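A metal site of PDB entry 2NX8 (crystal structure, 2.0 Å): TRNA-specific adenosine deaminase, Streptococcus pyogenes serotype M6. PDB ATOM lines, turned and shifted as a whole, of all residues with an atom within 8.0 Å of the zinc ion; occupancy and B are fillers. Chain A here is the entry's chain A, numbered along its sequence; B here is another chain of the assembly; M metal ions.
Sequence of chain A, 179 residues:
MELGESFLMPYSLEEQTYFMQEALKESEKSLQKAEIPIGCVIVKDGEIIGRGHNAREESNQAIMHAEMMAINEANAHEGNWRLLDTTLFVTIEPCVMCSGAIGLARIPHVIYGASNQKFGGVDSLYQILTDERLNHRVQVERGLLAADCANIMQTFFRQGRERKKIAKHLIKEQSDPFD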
ATOM      1  N   ILE A  38      13.962   7.135 -19.422  1.00  0.00           N
ATOM      2  CA  ILE A  38      13.299   7.904 -20.469  1.00  0.00           C
ATOM      3  C   ILE A  38      11.943   8.324 -19.911  1.00  0.00           C
ATOM      4  O   ILE A  38      11.226   7.510 -19.333  1.00  0.00           O
ATOM      5  CB  ILE A  38      13.089   7.066 -21.759  1.00  0.00           C
ATOM      6  CG1 ILE A  38      14.446   6.771 -22.398  1.00  0.00           C
ATOM      7  CG2 ILE A  38      12.199   7.812 -22.740  1.00  0.00           C
ATOM      8  CD1 ILE A  38      14.361   5.955 -23.658  1.00  0.00           C
ATOM      9  N   ASN A  54       9.671   4.730 -18.690  1.00  0.00           N
ATOM     10  CA  ASN A  54       9.878   3.330 -19.019  1.00  0.00           C
ATOM     11  C   ASN A  54       9.731   2.478 -17.763  1.00  0.00           C
ATOM     12  O   ASN A  54      10.323   2.793 -16.717  1.00  0.00           O
ATOM     13  CB  ASN A  54      11.265   3.110 -19.629  1.00  0.00           C
ATOM     14  CG  ASN A  54      11.322   3.479 -21.104  1.00  0.00           C
ATOM     15  OD1 ASN A  54      12.165   2.980 -21.847  1.00  0.00           O
ATOM     16  ND2 ASN A  54      10.434   4.364 -21.520  1.00  0.00           N
ATOM     17  N   ALA A  62       6.069  -5.599 -22.278  1.00  0.00           N
ATOM     18  CA  ALA A  62       7.001  -5.243 -23.343  1.00  0.00           C
ATOM     19  C   ALA A  62       6.736  -3.894 -24.010  1.00  0.00           C
ATOM     20  O   ALA A  62       7.643  -3.296 -24.569  1.00  0.00           O
ATOM     21  CB  ALA A  62       7.011  -6.330 -24.399  1.00  0.00           C
ATOM     22  N   ILE A  63       5.491  -3.426 -23.953  1.00  0.00           N
ATOM     23  CA  ILE A  63       5.124  -2.151 -24.586  1.00  0.00           C
ATOM     24  C   ILE A  63       5.188  -0.966 -23.636  1.00  0.00           C
ATOM     25  O   ILE A  63       4.900   0.162 -24.032  1.00  0.00           O
ATOM     26  CB  ILE A  63       3.688  -2.169 -25.119  1.00  0.00           C
ATOM     27  CG1 ILE A  63       2.703  -2.085 -23.947  1.00  0.00           C
ATOM     28  CG2 ILE A  63       3.428  -3.458 -25.920  1.00  0.00           C
ATOM     29  CD1 ILE A  63       1.238  -1.913 -24.371  1.00  0.00           C
ATOM     30  N   MET A  64       5.576  -1.217 -22.381  1.00  0.00           N
ATOM     31  CA  MET A  64       5.591  -0.169 -21.381  1.00  0.00           C
ATOM     32  C   MET A  64       6.717   0.857 -21.442  1.00  0.00           C
ATOM     33  O   MET A  64       7.485   1.023 -20.486  1.00  0.00           O
ATOM     34  CB  MET A  64       5.531  -0.797 -19.980  1.00  0.00           C
ATOM     35  CG  MET A  64       5.018   0.156 -18.917  1.00  0.00           C
ATOM     36  SD  MET A  64       3.472   0.954 -19.432  1.00  0.00           S
ATOM     37  CE  MET A  64       2.392  -0.467 -19.560  1.00  0.00           C
ATOM     38  N   HIS A  65       6.815   1.530 -22.579  1.00  0.00           N
ATOM     39  CA  HIS A  65       7.795   2.587 -22.759  1.00  0.00           C
ATOM     40  C   HIS A  65       7.116   3.856 -22.262  1.00  0.00           C
ATOM     41  O   HIS A  65       5.890   3.887 -22.132  1.00  0.00           O
ATOM     42  CB  HIS A  65       8.177   2.749 -24.223  1.00  0.00           C
ATOM     43  CG  HIS A  65       9.192   1.756 -24.691  1.00  0.00           C
ATOM     44  ND1 HIS A  65       9.813   1.839 -25.911  1.00  0.00           N
ATOM     45  CD2 HIS A  65       9.718   0.669 -24.083  1.00  0.00           C
ATOM     46  CE1 HIS A  65      10.675   0.847 -26.045  1.00  0.00           C
ATOM     47  NE2 HIS A  65      10.638   0.124 -24.945  1.00  0.00           N
ATOM     48  N   ALA A  66       7.906   4.888 -21.993  1.00  0.00           N
ATOM     49  CA  ALA A  66       7.369   6.156 -21.509  1.00  0.00           C
ATOM     50  C   ALA A  66       6.231   6.726 -22.351  1.00  0.00           C
ATOM     51  O   ALA A  66       5.198   7.106 -21.818  1.00  0.00           O
ATOM     52  CB  ALA A  66       8.511   7.193 -21.392  1.00  0.00           C
ATOM     53  N   GLU A  67       6.431   6.785 -23.666  1.00  0.00           N
ATOM     54  CA  GLU A  67       5.417   7.334 -24.568  1.00  0.00           C
ATOM     55  C   GLU A  67       4.081   6.593 -24.520  1.00  0.00           C
ATOM     56  O   GLU A  67       3.014   7.211 -24.558  1.00  0.00           O
ATOM     57  CB  GLU A  67       5.908   7.351 -26.013  1.00  0.00           C
ATOM     58  CG  GLU A  67       7.246   8.028 -26.220  1.00  0.00           C
ATOM     59  CD  GLU A  67       8.422   7.072 -26.056  1.00  0.00           C
ATOM     60  OE1 GLU A  67       9.257   7.005 -26.983  1.00  0.00           O
ATOM     61  OE2 GLU A  67       8.525   6.410 -25.003  1.00  0.00           O
ATOM     62  N   MET A  68       4.157   5.261 -24.426  1.00  0.00           N
ATOM     63  CA  MET A  68       2.963   4.419 -24.380  1.00  0.00           C
ATOM     64  C   MET A  68       2.176   4.673 -23.095  1.00  0.00           C
ATOM     65  O   MET A  68       0.945   4.759 -23.112  1.00  0.00           O
ATOM     66  CB  MET A  68       3.344   2.939 -24.447  1.00  0.00           C
ATOM     67  CG  MET A  68       4.138   2.560 -25.696  1.00  0.00           C
ATOM     68  SD  MET A  68       3.243   2.973 -27.214  1.00  0.00           S
ATOM     69  CE  MET A  68       2.309   1.429 -27.471  1.00  0.00           C
ATOM     70  N   VAL A  90       9.273  14.048 -25.061  1.00  0.00           N
ATOM     71  CA  VAL A  90       9.914  12.806 -24.623  1.00  0.00           C
ATOM     72  C   VAL A  90      11.424  13.026 -24.633  1.00  0.00           C
ATOM     73  O   VAL A  90      11.985  13.577 -25.579  1.00  0.00           O
ATOM     74  CB  VAL A  90       9.516  11.621 -25.560  1.00  0.00           C
ATOM     75  CG1 VAL A  90       9.954  11.899 -26.982  1.00  0.00           C
ATOM     76  CG2 VAL A  90      10.137  10.330 -25.051  1.00  0.00           C
ATOM     77  N   ILE A  92      13.961  11.068 -25.068  1.00  0.00           N
ATOM     78  CA  ILE A  92      14.717  10.411 -26.130  1.00  0.00           C
ATOM     79  C   ILE A  92      13.820  10.163 -27.337  1.00  0.00           C
ATOM     80  O   ILE A  92      12.620   9.900 -27.168  1.00  0.00           O
ATOM     81  CB  ILE A  92      15.287   9.045 -25.663  1.00  0.00           C
ATOM     82  CG1 ILE A  92      16.229   9.244 -24.461  1.00  0.00           C
ATOM     83  CG2 ILE A  92      16.018   8.371 -26.809  1.00  0.00           C
ATOM     84  CD1 ILE A  92      17.531   9.982 -24.773  1.00  0.00           C
ATOM     85  N   GLU A  93      14.390  10.251 -28.529  1.00  0.00           N
ATOM     86  CA  GLU A  93      13.664  10.019 -29.779  1.00  0.00           C
ATOM     87  C   GLU A  93      12.890   8.694 -29.688  1.00  0.00           C
ATOM     88  O   GLU A  93      13.473   7.653 -29.424  1.00  0.00           O
ATOM     89  CB  GLU A  93      14.654   9.964 -30.943  1.00  0.00           C
ATOM     90  CG  GLU A  93      14.063   9.432 -32.247  1.00  0.00           C
ATOM     91  CD  GLU A  93      15.112   9.173 -33.304  1.00  0.00           C
ATOM     92  OE1 GLU A  93      16.321   9.173 -32.971  1.00  0.00           O
ATOM     93  OE2 GLU A  93      14.738   8.938 -34.472  1.00  0.00           O
ATOM     94  N   PRO A  94      11.569   8.734 -29.926  1.00  0.00           N
ATOM     95  CA  PRO A  94      10.738   7.513 -29.862  1.00  0.00           C
ATOM     96  C   PRO A  94      11.180   6.383 -30.785  1.00  0.00           C
ATOM     97  O   PRO A  94      11.626   6.609 -31.925  1.00  0.00           O
ATOM     98  CB  PRO A  94       9.341   8.026 -30.219  1.00  0.00           C
ATOM     99  CG  PRO A  94       9.353   9.442 -29.678  1.00  0.00           C
ATOM    100  CD  PRO A  94      10.724   9.930 -30.110  1.00  0.00           C
ATOM    101  N   CYS A  95      11.046   5.159 -30.295  1.00  0.00           N
ATOM    102  CA  CYS A  95      11.408   3.985 -31.073  1.00  0.00           C
ATOM    103  C   CYS A  95      10.292   3.769 -32.117  1.00  0.00           C
ATOM    104  O   CYS A  95       9.371   4.579 -32.229  1.00  0.00           O
ATOM    105  CB  CYS A  95      11.501   2.767 -30.157  1.00  0.00           C
ATOM    106  SG  CYS A  95       9.880   2.126 -29.600  1.00  0.00           S
ATOM    107  N   VAL A  96      10.399   2.691 -32.862  1.00  0.00           N
ATOM    108  CA  VAL A  96       9.410   2.365 -33.894  1.00  0.00           C
ATOM    109  C   VAL A  96       8.010   2.141 -33.323  1.00  0.00           C
ATOM    110  O   VAL A  96       7.031   2.644 -33.876  1.00  0.00           O
ATOM    111  CB  VAL A  96       9.862   1.124 -34.685  1.00  0.00           C
ATOM    112  CG1 VAL A  96       8.724   0.615 -35.567  1.00  0.00           C
ATOM    113  CG2 VAL A  96      11.064   1.475 -35.534  1.00  0.00           C
ATOM    114  N   MET A  97       7.910   1.402 -32.230  1.00  0.00           N
ATOM    115  CA  MET A  97       6.604   1.140 -31.632  1.00  0.00           C
ATOM    116  C   MET A  97       5.911   2.431 -31.183  1.00  0.00           C
ATOM    117  O   MET A  97       4.736   2.668 -31.486  1.00  0.00           O
ATOM    118  CB  MET A  97       6.734   0.203 -30.435  1.00  0.00           C
ATOM    119  CG  MET A  97       5.422  -0.021 -29.711  1.00  0.00           C
ATOM    120  SD  MET A  97       5.590  -0.856 -28.133  1.00  0.00           S
ATOM    121  CE  MET A  97       6.591   0.418 -27.204  1.00  0.00           C
ATOM    122  N   CYS A  98       6.628   3.261 -30.428  1.00  0.00           N
ATOM    123  CA  CYS A  98       6.051   4.490 -29.925  1.00  0.00           C
ATOM    124  C   CYS A  98       5.724   5.474 -31.035  1.00  0.00           C
ATOM    125  O   CYS A  98       4.700   6.168 -30.986  1.00  0.00           O
ATOM    126  CB  CYS A  98       6.992   5.113 -28.878  1.00  0.00           C
ATOM    127  SG  CYS A  98       7.102   4.099 -27.354  1.00  0.00           S
ATOM    128  N   SER A  99       6.574   5.541 -32.059  1.00  0.00           N
ATOM    129  CA  SER A  99       6.325   6.427 -33.177  1.00  0.00           C
ATOM    130  C   SER A  99       4.996   6.020 -33.820  1.00  0.00           C
ATOM    131  O   SER A  99       4.135   6.857 -34.092  1.00  0.00           O
ATOM    132  CB  SER A  99       7.442   6.316 -34.222  1.00  0.00           C
ATOM    133  OG  SER A  99       8.670   6.806 -33.713  1.00  0.00           O
ATOM    134  N   GLY A 100       4.832   4.718 -34.045  1.00  0.00           N
ATOM    135  CA  GLY A 100       3.599   4.224 -34.632  1.00  0.00           C
ATOM    136  C   GLY A 100       2.407   4.594 -33.772  1.00  0.00           C
ATOM    137  O   GLY A 100       1.354   4.988 -34.268  1.00  0.00           O
ATOM    138  N   ALA A 101       2.579   4.473 -32.454  1.00  0.00           N
ATOM    139  CA  ALA A 101       1.522   4.791 -31.509  1.00  0.00           C
ATOM    140  C   ALA A 101       1.180   6.287 -31.575  1.00  0.00           C
ATOM    141  O   ALA A 101       0.013   6.667 -31.567  1.00  0.00           O
ATOM    142  CB  ALA A 101       1.957   4.416 -30.101  1.00  0.00           C
ATOM    143  N   ILE A 102       2.212   7.121 -31.638  1.00  0.00           N
ATOM    144  CA  ILE A 102       2.037   8.560 -31.719  1.00  0.00           C
ATOM    145  C   ILE A 102       1.215   8.926 -32.964  1.00  0.00           C
ATOM    146  O   ILE A 102       0.363   9.813 -32.931  1.00  0.00           O
ATOM    147  CB  ILE A 102       3.418   9.258 -31.763  1.00  0.00           C
ATOM    148  CG1 ILE A 102       4.119   9.065 -30.415  1.00  0.00           C
ATOM    149  CG2 ILE A 102       3.270  10.733 -32.114  1.00  0.00           C
ATOM    150  CD1 ILE A 102       5.568   9.550 -30.382  1.00  0.00           C
ATOM    151  N   ASN A 116      17.917   8.781 -30.810  1.00  0.00           N
ATOM    152  CA  ASN A 116      18.084   7.365 -30.514  1.00  0.00           C
ATOM    153  C   ASN A 116      18.667   6.740 -31.778  1.00  0.00           C
ATOM    154  O   ASN A 116      17.937   6.295 -32.668  1.00  0.00           O
ATOM    155  CB  ASN A 116      16.731   6.749 -30.181  1.00  0.00           C
ATOM    156  CG  ASN A 116      16.857   5.371 -29.553  1.00  0.00           C
ATOM    157  OD1 ASN A 116      15.872   4.817 -29.069  1.00  0.00           O
ATOM    158  ND2 ASN A 116      18.057   4.807 -29.559  1.00  0.00           N
ATOM    159  N   PHE A 119      17.610   2.687 -31.985  1.00  0.00           N
ATOM    160  CA  PHE A 119      16.225   2.277 -32.194  1.00  0.00           C
ATOM    161  C   PHE A 119      15.307   3.412 -32.625  1.00  0.00           C
ATOM    162  O   PHE A 119      14.096   3.225 -32.728  1.00  0.00           O
ATOM    163  CB  PHE A 119      15.659   1.639 -30.912  1.00  0.00           C
ATOM    164  CG  PHE A 119      16.600   0.682 -30.224  1.00  0.00           C
ATOM    165  CD1 PHE A 119      17.534   1.136 -29.290  1.00  0.00           C
ATOM    166  CD2 PHE A 119      16.578  -0.684 -30.530  1.00  0.00           C
ATOM    167  CE1 PHE A 119      18.423   0.259 -28.673  1.00  0.00           C
ATOM    168  CE2 PHE A 119      17.460  -1.573 -29.918  1.00  0.00           C
ATOM    169  CZ  PHE A 119      18.385  -1.096 -28.986  1.00  0.00           C
ATOM    170  N   GLY B 100       6.588  -3.012 -34.100  1.00  0.00           N
ATOM    171  CA  GLY B 100       7.608  -2.570 -33.166  1.00  0.00           C
ATOM    172  C   GLY B 100       7.448  -3.262 -31.827  1.00  0.00           C
ATOM    173  O   GLY B 100       8.419  -3.676 -31.199  1.00  0.00           O
ATOM    174  N   LEU B 104       9.914  -5.820 -29.650  1.00  0.00           N
ATOM    175  CA  LEU B 104      10.300  -5.550 -28.261  1.00  0.00           C
ATOM    176  C   LEU B 104       9.978  -6.729 -27.327  1.00  0.00           C
ATOM    177  O   LEU B 104      10.646  -6.913 -26.308  1.00  0.00           O
ATOM    178  CB  LEU B 104       9.586  -4.289 -27.762  1.00  0.00           C
ATOM    179  CG  LEU B 104      10.030  -2.960 -28.381  1.00  0.00           C
ATOM    180  CD1 LEU B 104       9.060  -1.864 -27.980  1.00  0.00           C
ATOM    181  CD2 LEU B 104      11.454  -2.626 -27.933  1.00  0.00           C
HETATM  182 ZN    ZN M   1       9.210   3.086 -27.587  1.00  0.00          ZN
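SG of Cys 95 sits close to N of Met 97, 3.4 Å away. O of Cys 95 is in hydrogen-bond range of OG of Ser 99, at 2.8 Å. SG of Cys 98 lies close to OE2 of Glu 67.
Merely in contact with the zinc ion: Glu 67 (3.97 Å) and Met 97 (3.8 Å). Of the 25 residues printed, 5 come within 4 Å of the zinc ion. Along chain A the residues within 4 Å of the zinc ion span positions 65 to 98.
ND1 of His 65 is bound to the zinc ion, 2.2 Å away. SG of Cys 95 is bound to the zinc ion (2.3 Å). The side-chain sulfur (SG) of Cys 98 binds the zinc ion, at 2.4 Å.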
